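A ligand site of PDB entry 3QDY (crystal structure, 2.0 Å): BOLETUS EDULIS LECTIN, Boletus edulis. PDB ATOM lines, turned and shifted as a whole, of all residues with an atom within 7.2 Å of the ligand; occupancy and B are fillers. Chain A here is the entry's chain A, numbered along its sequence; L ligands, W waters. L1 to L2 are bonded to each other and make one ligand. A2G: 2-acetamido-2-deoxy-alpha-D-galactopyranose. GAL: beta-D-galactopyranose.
Residues that only touch the ligand: His 72, Tyr 29, Tyr 74 and Tyr 98. Hydrophobic or aromatic side chains within 4 Å of the ligand: Tyr 29, His 72, Tyr 74 and Tyr 98. Within 4 Å of the ligand: Tyr 29, Ala 30, Ser 49, Gly 50, His 72, Asn 73, Tyr 74, Tyr 98 and Arg 107. The nearest printed residue that does not touch the ligand is Val 71 (4.4 Å).
An oxygen (O6) of A2G L1 lies within hydrogen-bond range of the guanidinium group (NH1) of Arg 107, at 3.4 Å. O4 of GAL L2 sits at hydrogen-bond distance from N of Ala 30 (2.9 Å). The backbone carbonyl oxygen (O) of Gly 50 lies within hydrogen-bond range of an oxygen (O4) of A2G L1 (2.7 Å). The side-chain amide oxygen (OD1) of Asn 73 sits close to a nitrogen (N2) of A2G L1, 3.4 Å away. An oxygen (O7) of A2G L1 is in hydrogen-bond range of the side-chain hydroxyl (OG) of Ser 49 (2.7 Å). The backbone NH of Gly 50 is in hydrogen-bond range of an oxygen (O7) of A2G L1 (3.3 Å). An oxygen (O7) of A2G L1 sits at hydrogen-bond distance from the backbone NH of Asn 73 (2.9 Å). The backbone carbonyl oxygen of Ser 49 is in hydrogen-bond range of an oxygen (O2) of GAL L2.
The backbone NH (N) of Gly 50 is in hydrogen-bond range of the backbone carbonyl oxygen (O) of Val 71. The side-chain hydroxyl of Ser 49 lies within hydrogen-bond range of the backbone NH of Tyr 74, 2.8 Å away. The guanidinium group (NE) of Arg 107 is in hydrogen-bond range of the backbone carbonyl oxygen (O) of Tyr 97 (2.7 Å). The backbone carbonyl oxygen (O) of Tyr 29 lies close to the side-chain hydroxyl (OG1) of Thr 51 (3.4 Å). OH of Tyr 29 is in hydrogen-bond range of OD1 of Asn 99, at 3.5 Å. The backbone NH of Asn 73 lies within hydrogen-bond range of the side-chain hydroxyl of Ser 49 (3.3 Å). The backbone NH (N) of Gly 48 lies within hydrogen-bond range of the backbone carbonyl oxygen (O) of Ala 30 (3.4 Å). NH1 of Arg 107 lies close to NE2 of His 72, 3.2 Å away.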
ATOM      1  N   PHE A  27      -3.612 -11.100  11.504  1.00  0.00           N
ATOM      2  CA  PHE A  27      -3.671  -9.868  12.287  1.00  0.00           C
ATOM      3  C   PHE A  27      -3.333  -8.668  11.405  1.00  0.00           C
ATOM      4  O   PHE A  27      -2.639  -8.804  10.396  1.00  0.00           O
ATOM      5  CB  PHE A  27      -2.742  -9.953  13.497  1.00  0.00           C
ATOM      6  CG  PHE A  27      -3.049  -8.935  14.575  1.00  0.00           C
ATOM      7  CD1 PHE A  27      -2.190  -7.877  14.810  1.00  0.00           C
ATOM      8  CD2 PHE A  27      -4.210  -9.037  15.328  1.00  0.00           C
ATOM      9  CE1 PHE A  27      -2.477  -6.939  15.800  1.00  0.00           C
ATOM     10  CE2 PHE A  27      -4.508  -8.105  16.315  1.00  0.00           C
ATOM     11  CZ  PHE A  27      -3.642  -7.050  16.554  1.00  0.00           C
ATOM     12  N   HIS A  28      -3.829  -7.502  11.789  1.00  0.00           N
ATOM     13  CA  HIS A  28      -3.835  -6.339  10.903  1.00  0.00           C
ATOM     14  C   HIS A  28      -2.550  -5.500  10.916  1.00  0.00           C
ATOM     15  O   HIS A  28      -2.428  -4.551  10.139  1.00  0.00           O
ATOM     16  CB  HIS A  28      -5.055  -5.447  11.175  1.00  0.00           C
ATOM     17  CG  HIS A  28      -5.058  -4.824  12.536  1.00  0.00           C
ATOM     18  ND1 HIS A  28      -5.639  -5.422  13.634  1.00  0.00           N
ATOM     19  CD2 HIS A  28      -4.550  -3.641  12.968  1.00  0.00           C
ATOM     20  CE1 HIS A  28      -5.489  -4.633  14.689  1.00  0.00           C
ATOM     21  NE2 HIS A  28      -4.827  -3.552  14.318  1.00  0.00           N
ATOM     22  N   TYR A  29      -1.609  -5.839  11.790  1.00  0.00           N
ATOM     23  CA  TYR A  29      -0.335  -5.123  11.832  1.00  0.00           C
ATOM     24  C   TYR A  29       0.508  -5.421  10.600  1.00  0.00           C
ATOM     25  O   TYR A  29       0.196  -6.330   9.830  1.00  0.00           O
ATOM     26  CB  TYR A  29       0.470  -5.488  13.092  1.00  0.00           C
ATOM     27  CG  TYR A  29      -0.027  -4.849  14.366  1.00  0.00           C
ATOM     28  CD1 TYR A  29       0.466  -5.256  15.603  1.00  0.00           C
ATOM     29  CD2 TYR A  29      -0.988  -3.848  14.341  1.00  0.00           C
ATOM     30  CE1 TYR A  29       0.025  -4.683  16.776  1.00  0.00           C
ATOM     31  CE2 TYR A  29      -1.442  -3.260  15.503  1.00  0.00           C
ATOM     32  CZ  TYR A  29      -0.930  -3.680  16.719  1.00  0.00           C
ATOM     33  OH  TYR A  29      -1.379  -3.103  17.887  1.00  0.00           O
ATOM     34  N   ALA A  30       1.567  -4.637  10.425  1.00  0.00           N
ATOM     35  CA  ALA A  30       2.553  -4.879   9.359  1.00  0.00           C
ATOM     36  C   ALA A  30       1.938  -5.021   7.974  1.00  0.00           C
ATOM     37  O   ALA A  30       2.460  -5.751   7.121  1.00  0.00           O
ATOM     38  CB  ALA A  30       3.423  -6.093   9.699  1.00  0.00           C
ATOM     39  N   ASN A  31       0.824  -4.333   7.747  1.00  0.00           N
ATOM     40  CA  ASN A  31       0.176  -4.333   6.446  1.00  0.00           C
ATOM     41  C   ASN A  31      -0.558  -5.642   6.172  1.00  0.00           C
ATOM     42  O   ASN A  31      -0.741  -6.035   5.015  1.00  0.00           O
ATOM     43  CB  ASN A  31       1.206  -4.058   5.346  1.00  0.00           C
ATOM     44  CG  ASN A  31       0.743  -2.993   4.385  1.00  0.00           C
ATOM     45  OD1 ASN A  31       0.253  -1.935   4.799  1.00  0.00           O
ATOM     46  ND2 ASN A  31       0.896  -3.250   3.090  1.00  0.00           N
ATOM     47  N   GLY A  32      -0.980  -6.316   7.238  1.00  0.00           N
ATOM     48  CA  GLY A  32      -1.752  -7.550   7.103  1.00  0.00           C
ATOM     49  C   GLY A  32      -0.985  -8.700   6.495  1.00  0.00           C
ATOM     50  O   GLY A  32       0.236  -8.796   6.641  1.00  0.00           O
ATOM     51  N   GLY A  48       5.321  -7.511   6.390  1.00  0.00           N
ATOM     52  CA  GLY A  48       6.541  -7.119   7.089  1.00  0.00           C
ATOM     53  C   GLY A  48       6.619  -7.762   8.456  1.00  0.00           C
ATOM     54  O   GLY A  48       5.762  -8.569   8.816  1.00  0.00           O
ATOM     55  N   SER A  49       7.642  -7.414   9.226  1.00  0.00           N
ATOM     56  CA  SER A  49       7.757  -7.918  10.592  1.00  0.00           C
ATOM     57  C   SER A  49       6.748  -7.226  11.506  1.00  0.00           C
ATOM     58  O   SER A  49       6.509  -6.023  11.377  1.00  0.00           O
ATOM     59  CB  SER A  49       9.173  -7.698  11.127  1.00  0.00           C
ATOM     60  OG  SER A  49       9.292  -8.152  12.476  1.00  0.00           O
ATOM     61  N   GLY A  50       6.141  -7.991  12.414  1.00  0.00           N
ATOM     62  CA  GLY A  50       5.271  -7.400  13.423  1.00  0.00           C
ATOM     63  C   GLY A  50       3.826  -7.851  13.384  1.00  0.00           C
ATOM     64  O   GLY A  50       2.982  -7.293  14.085  1.00  0.00           O
ATOM     65  N   THR A  51       3.516  -8.858  12.570  1.00  0.00           N
ATOM     66  CA  THR A  51       2.167  -9.410  12.573  1.00  0.00           C
ATOM     67  C   THR A  51       2.190 -10.929  12.636  1.00  0.00           C
ATOM     68  O   THR A  51       3.244 -11.534  12.807  1.00  0.00           O
ATOM     69  CB  THR A  51       1.316  -8.902  11.379  1.00  0.00           C
ATOM     70  OG1 THR A  51      -0.058  -9.202  11.611  1.00  0.00           O
ATOM     71  CG2 THR A  51       1.775  -9.542  10.066  1.00  0.00           C
ATOM     72  N   VAL A  71       5.988 -13.138  13.022  1.00  0.00           N
ATOM     73  CA  VAL A  71       7.337 -12.593  13.101  1.00  0.00           C
ATOM     74  C   VAL A  71       7.313 -11.385  14.022  1.00  0.00           C
ATOM     75  O   VAL A  71       6.563 -10.425  13.802  1.00  0.00           O
ATOM     76  CB  VAL A  71       7.870 -12.183  11.709  1.00  0.00           C
ATOM     77  CG1 VAL A  71       9.271 -11.585  11.837  1.00  0.00           C
ATOM     78  CG2 VAL A  71       7.897 -13.385  10.765  1.00  0.00           C
ATOM     79  N   HIS A  72       8.132 -11.429  15.068  1.00  0.00           N
ATOM     80  CA  HIS A  72       8.197 -10.362  16.043  1.00  0.00           C
ATOM     81  C   HIS A  72       9.615  -9.772  16.111  1.00  0.00           C
ATOM     82  O   HIS A  72      10.550 -10.447  16.521  1.00  0.00           O
ATOM     83  CB  HIS A  72       7.769 -10.866  17.421  1.00  0.00           C
ATOM     84  CG  HIS A  72       7.904  -9.833  18.507  1.00  0.00           C
ATOM     85  ND1 HIS A  72       8.801  -9.979  19.543  1.00  0.00           N
ATOM     86  CD2 HIS A  72       7.277  -8.652  18.705  1.00  0.00           C
ATOM     87  CE1 HIS A  72       8.718  -8.921  20.345  1.00  0.00           C
ATOM     88  NE2 HIS A  72       7.791  -8.109  19.854  1.00  0.00           N
ATOM     89  N   ASN A  73       9.746  -8.520  15.685  1.00  0.00           N
ATOM     90  CA  ASN A  73      11.048  -7.866  15.636  1.00  0.00           C
ATOM     91  C   ASN A  73      12.067  -8.664  14.833  1.00  0.00           C
ATOM     92  O   ASN A  73      13.226  -8.788  15.227  1.00  0.00           O
ATOM     93  CB  ASN A  73      11.566  -7.555  17.044  1.00  0.00           C
ATOM     94  CG  ASN A  73      10.842  -6.375  17.681  1.00  0.00           C
ATOM     95  OD1 ASN A  73      10.379  -5.473  16.985  1.00  0.00           O
ATOM     96  ND2 ASN A  73      10.747  -6.383  19.006  1.00  0.00           N
ATOM     97  N   TYR A  74      11.616  -9.219  13.714  1.00  0.00           N
ATOM     98  CA  TYR A  74      12.500  -9.876  12.746  1.00  0.00           C
ATOM     99  C   TYR A  74      12.881 -11.309  13.122  1.00  0.00           C
ATOM    100  O   TYR A  74      13.702 -11.929  12.445  1.00  0.00           O
ATOM    101  CB  TYR A  74      13.739  -9.009  12.490  1.00  0.00           C
ATOM    102  CG  TYR A  74      13.380  -7.564  12.233  1.00  0.00           C
ATOM    103  CD1 TYR A  74      13.615  -6.587  13.187  1.00  0.00           C
ATOM    104  CD2 TYR A  74      12.770  -7.186  11.038  1.00  0.00           C
ATOM    105  CE1 TYR A  74      13.278  -5.268  12.963  1.00  0.00           C
ATOM    106  CE2 TYR A  74      12.428  -5.867  10.801  1.00  0.00           C
ATOM    107  CZ  TYR A  74      12.688  -4.911  11.761  1.00  0.00           C
ATOM    108  OH  TYR A  74      12.351  -3.605  11.530  1.00  0.00           O
ATOM    109  N   LYS A  75      12.270 -11.823  14.176  1.00  0.00           N
ATOM    110  CA  LYS A  75      12.493 -13.205  14.569  1.00  0.00           C
ATOM    111  C   LYS A  75      11.165 -13.950  14.607  1.00  0.00           C
ATOM    112  O   LYS A  75      10.144 -13.386  15.025  1.00  0.00           O
ATOM    113  CB  LYS A  75      13.156 -13.275  15.949  1.00  0.00           C
ATOM    114  CG  LYS A  75      14.581 -12.737  15.993  1.00  0.00           C
ATOM    115  CD  LYS A  75      15.148 -12.836  17.400  1.00  0.00           C
ATOM    116  CE  LYS A  75      16.566 -12.312  17.470  1.00  0.00           C
ATOM    117  NZ  LYS A  75      17.068 -12.306  18.868  1.00  0.00           N
ATOM    118  N   TYR A  97      -2.723 -11.843  21.293  1.00  0.00           N
ATOM    119  CA  TYR A  97      -1.264 -11.794  21.291  1.00  0.00           C
ATOM    120  C   TYR A  97      -0.750 -10.344  21.249  1.00  0.00           C
ATOM    121  O   TYR A  97       0.449 -10.108  21.276  1.00  0.00           O
ATOM    122  CB  TYR A  97      -0.688 -12.594  20.120  1.00  0.00           C
ATOM    123  CG  TYR A  97      -0.887 -14.090  20.253  1.00  0.00           C
ATOM    124  CD1 TYR A  97      -1.990 -14.721  19.690  1.00  0.00           C
ATOM    125  CD2 TYR A  97       0.033 -14.874  20.948  1.00  0.00           C
ATOM    126  CE1 TYR A  97      -2.176 -16.078  19.823  1.00  0.00           C
ATOM    127  CE2 TYR A  97      -0.157 -16.240  21.083  1.00  0.00           C
ATOM    128  CZ  TYR A  97      -1.265 -16.838  20.506  1.00  0.00           C
ATOM    129  OH  TYR A  97      -1.460 -18.193  20.635  1.00  0.00           O
ATOM    130  N   TYR A  98      -1.673  -9.393  21.167  1.00  0.00           N
ATOM    131  CA  TYR A  98      -1.295  -8.000  21.032  1.00  0.00           C
ATOM    132  C   TYR A  98      -2.026  -7.095  22.031  1.00  0.00           C
ATOM    133  O   TYR A  98      -2.898  -7.550  22.771  1.00  0.00           O
ATOM    134  CB  TYR A  98      -1.532  -7.521  19.590  1.00  0.00           C
ATOM    135  CG  TYR A  98      -0.790  -8.336  18.563  1.00  0.00           C
ATOM    136  CD1 TYR A  98      -1.327  -9.499  18.043  1.00  0.00           C
ATOM    137  CD2 TYR A  98       0.468  -7.944  18.122  1.00  0.00           C
ATOM    138  CE1 TYR A  98      -0.641 -10.261  17.110  1.00  0.00           C
ATOM    139  CE2 TYR A  98       1.166  -8.691  17.177  1.00  0.00           C
ATOM    140  CZ  TYR A  98       0.605  -9.850  16.681  1.00  0.00           C
ATOM    141  OH  TYR A  98       1.299 -10.594  15.745  1.00  0.00           O
ATOM    142  N   ASN A  99      -1.665  -5.822  22.048  1.00  0.00           N
ATOM    143  CA  ASN A  99      -2.312  -4.853  22.932  1.00  0.00           C
ATOM    144  C   ASN A  99      -2.340  -5.335  24.379  1.00  0.00           C
ATOM    145  O   ASN A  99      -3.349  -5.194  25.072  1.00  0.00           O
ATOM    146  CB  ASN A  99      -3.730  -4.566  22.439  1.00  0.00           C
ATOM    147  CG  ASN A  99      -3.747  -3.941  21.059  1.00  0.00           C
ATOM    148  OD1 ASN A  99      -3.206  -2.857  20.843  1.00  0.00           O
ATOM    149  ND2 ASN A  99      -4.383  -4.628  20.106  1.00  0.00           N
ATOM    150  N   ASN A 100      -1.224  -5.919  24.820  1.00  0.00           N
ATOM    151  CA  ASN A 100      -1.104  -6.415  26.185  1.00  0.00           C
ATOM    152  C   ASN A 100      -2.135  -7.482  26.521  1.00  0.00           C
ATOM    153  O   ASN A 100      -2.533  -7.641  27.672  1.00  0.00           O
ATOM    154  CB  ASN A 100      -1.202  -5.259  27.185  1.00  0.00           C
ATOM    155  CG  ASN A 100      -0.068  -4.270  27.046  1.00  0.00           C
ATOM    156  OD1 ASN A 100       1.107  -4.643  27.079  1.00  0.00           O
ATOM    157  ND2 ASN A 100      -0.410  -2.992  26.892  1.00  0.00           N
ATOM    158  N   ALA A 104       0.331 -12.240  24.674  1.00  0.00           N
ATOM    159  CA  ALA A 104       1.443 -11.451  24.164  1.00  0.00           C
ATOM    160  C   ALA A 104       2.796 -11.961  24.677  1.00  0.00           C
ATOM    161  O   ALA A 104       3.813 -11.816  23.997  1.00  0.00           O
ATOM    162  CB  ALA A 104       1.257  -9.984  24.521  1.00  0.00           C
ATOM    163  N   ARG A 107       4.311 -14.639  22.425  1.00  0.00           N
ATOM    164  CA  ARG A 107       4.833 -14.013  21.213  1.00  0.00           C
ATOM    165  C   ARG A 107       6.201 -13.362  21.433  1.00  0.00           C
ATOM    166  O   ARG A 107       7.074 -13.408  20.568  1.00  0.00           O
ATOM    167  CB  ARG A 107       3.867 -12.948  20.670  1.00  0.00           C
ATOM    168  CG  ARG A 107       4.523 -11.974  19.695  1.00  0.00           C
ATOM    169  CD  ARG A 107       3.557 -10.921  19.145  1.00  0.00           C
ATOM    170  NE  ARG A 107       2.905 -10.133  20.186  1.00  0.00           N
ATOM    171  CZ  ARG A 107       3.445  -9.059  20.774  1.00  0.00           C
ATOM    172  NH1 ARG A 107       4.647  -8.647  20.428  1.00  0.00           N
ATOM    173  NH2 ARG A 107       2.768  -8.412  21.706  1.00  0.00           N
ATOM    174  N   GLU A 108       6.372 -12.731  22.589  1.00  0.00           N
ATOM    175  CA  GLU A 108       7.601 -12.004  22.895  1.00  0.00           C
ATOM    176  C   GLU A 108       8.810 -12.935  23.056  1.00  0.00           C
ATOM    177  O   GLU A 108       9.952 -12.503  22.918  1.00  0.00           O
ATOM    178  CB  GLU A 108       7.404 -11.118  24.124  1.00  0.00           C
ATOM    179  CG  GLU A 108       6.481  -9.933  23.864  1.00  0.00           C
ATOM    180  CD  GLU A 108       5.942  -9.287  25.130  1.00  0.00           C
ATOM    181  OE1 GLU A 108       6.019  -9.916  26.205  1.00  0.00           O
ATOM    182  OE2 GLU A 108       5.432  -8.156  25.040  1.00  0.00           O
HETATM  183  O5  A2G L   1       5.757  -5.633  18.347  1.00  0.00           O
HETATM  184  C1  A2G L   1       6.876  -5.164  17.556  1.00  0.00           C
HETATM  185  O1  A2G L   1       7.255  -3.863  18.016  1.00  0.00           O
HETATM  186  C2  A2G L   1       6.513  -5.093  16.062  1.00  0.00           C
HETATM  187  N2  A2G L   1       7.621  -4.503  15.303  1.00  0.00           N
HETATM  188  C3  A2G L   1       5.261  -4.238  15.866  1.00  0.00           C
HETATM  189  O3  A2G L   1       4.843  -4.298  14.499  1.00  0.00           O
HETATM  190  C4  A2G L   1       4.149  -4.744  16.775  1.00  0.00           C
HETATM  191  O4  A2G L   1       3.781  -6.071  16.386  1.00  0.00           O
HETATM  192  C5  A2G L   1       4.628  -4.752  18.226  1.00  0.00           C
HETATM  193  C6  A2G L   1       3.469  -5.219  19.114  1.00  0.00           C
HETATM  194  O6  A2G L   1       3.899  -5.298  20.479  1.00  0.00           O
HETATM  195  C7  A2G L   1       8.383  -5.240  14.507  1.00  0.00           C
HETATM  196  O7  A2G L   1       8.261  -6.453  14.374  1.00  0.00           O
HETATM  197  C8  A2G L   1       9.496  -4.472  13.765  1.00  0.00           C
HETATM  198  C1  GAL L   2       4.394  -3.037  13.986  1.00  0.00           C
HETATM  199  C2  GAL L   2       4.344  -3.145  12.460  1.00  0.00           C
HETATM  200  C3  GAL L   2       3.895  -1.822  11.856  1.00  0.00           C
HETATM  201  C4  GAL L   2       2.586  -1.389  12.500  1.00  0.00           C
HETATM  202  C5  GAL L   2       2.725  -1.357  14.011  1.00  0.00           C
HETATM  203  C6  GAL L   2       1.400  -0.960  14.661  1.00  0.00           C
HETATM  204  O2  GAL L   2       5.620  -3.514  11.962  1.00  0.00           O
HETATM  205  O3  GAL L   2       3.717  -1.948  10.466  1.00  0.00           O
HETATM  206  O4  GAL L   2       1.567  -2.308  12.146  1.00  0.00           O
HETATM  207  O5  GAL L   2       3.135  -2.631  14.478  1.00  0.00           O
HETATM  208  O6  GAL L   2       1.597  -0.681  16.026  1.00  0.00           O
HETATM  209  O   HOH W   1       5.079  -8.471  16.802  1.00  0.00           O
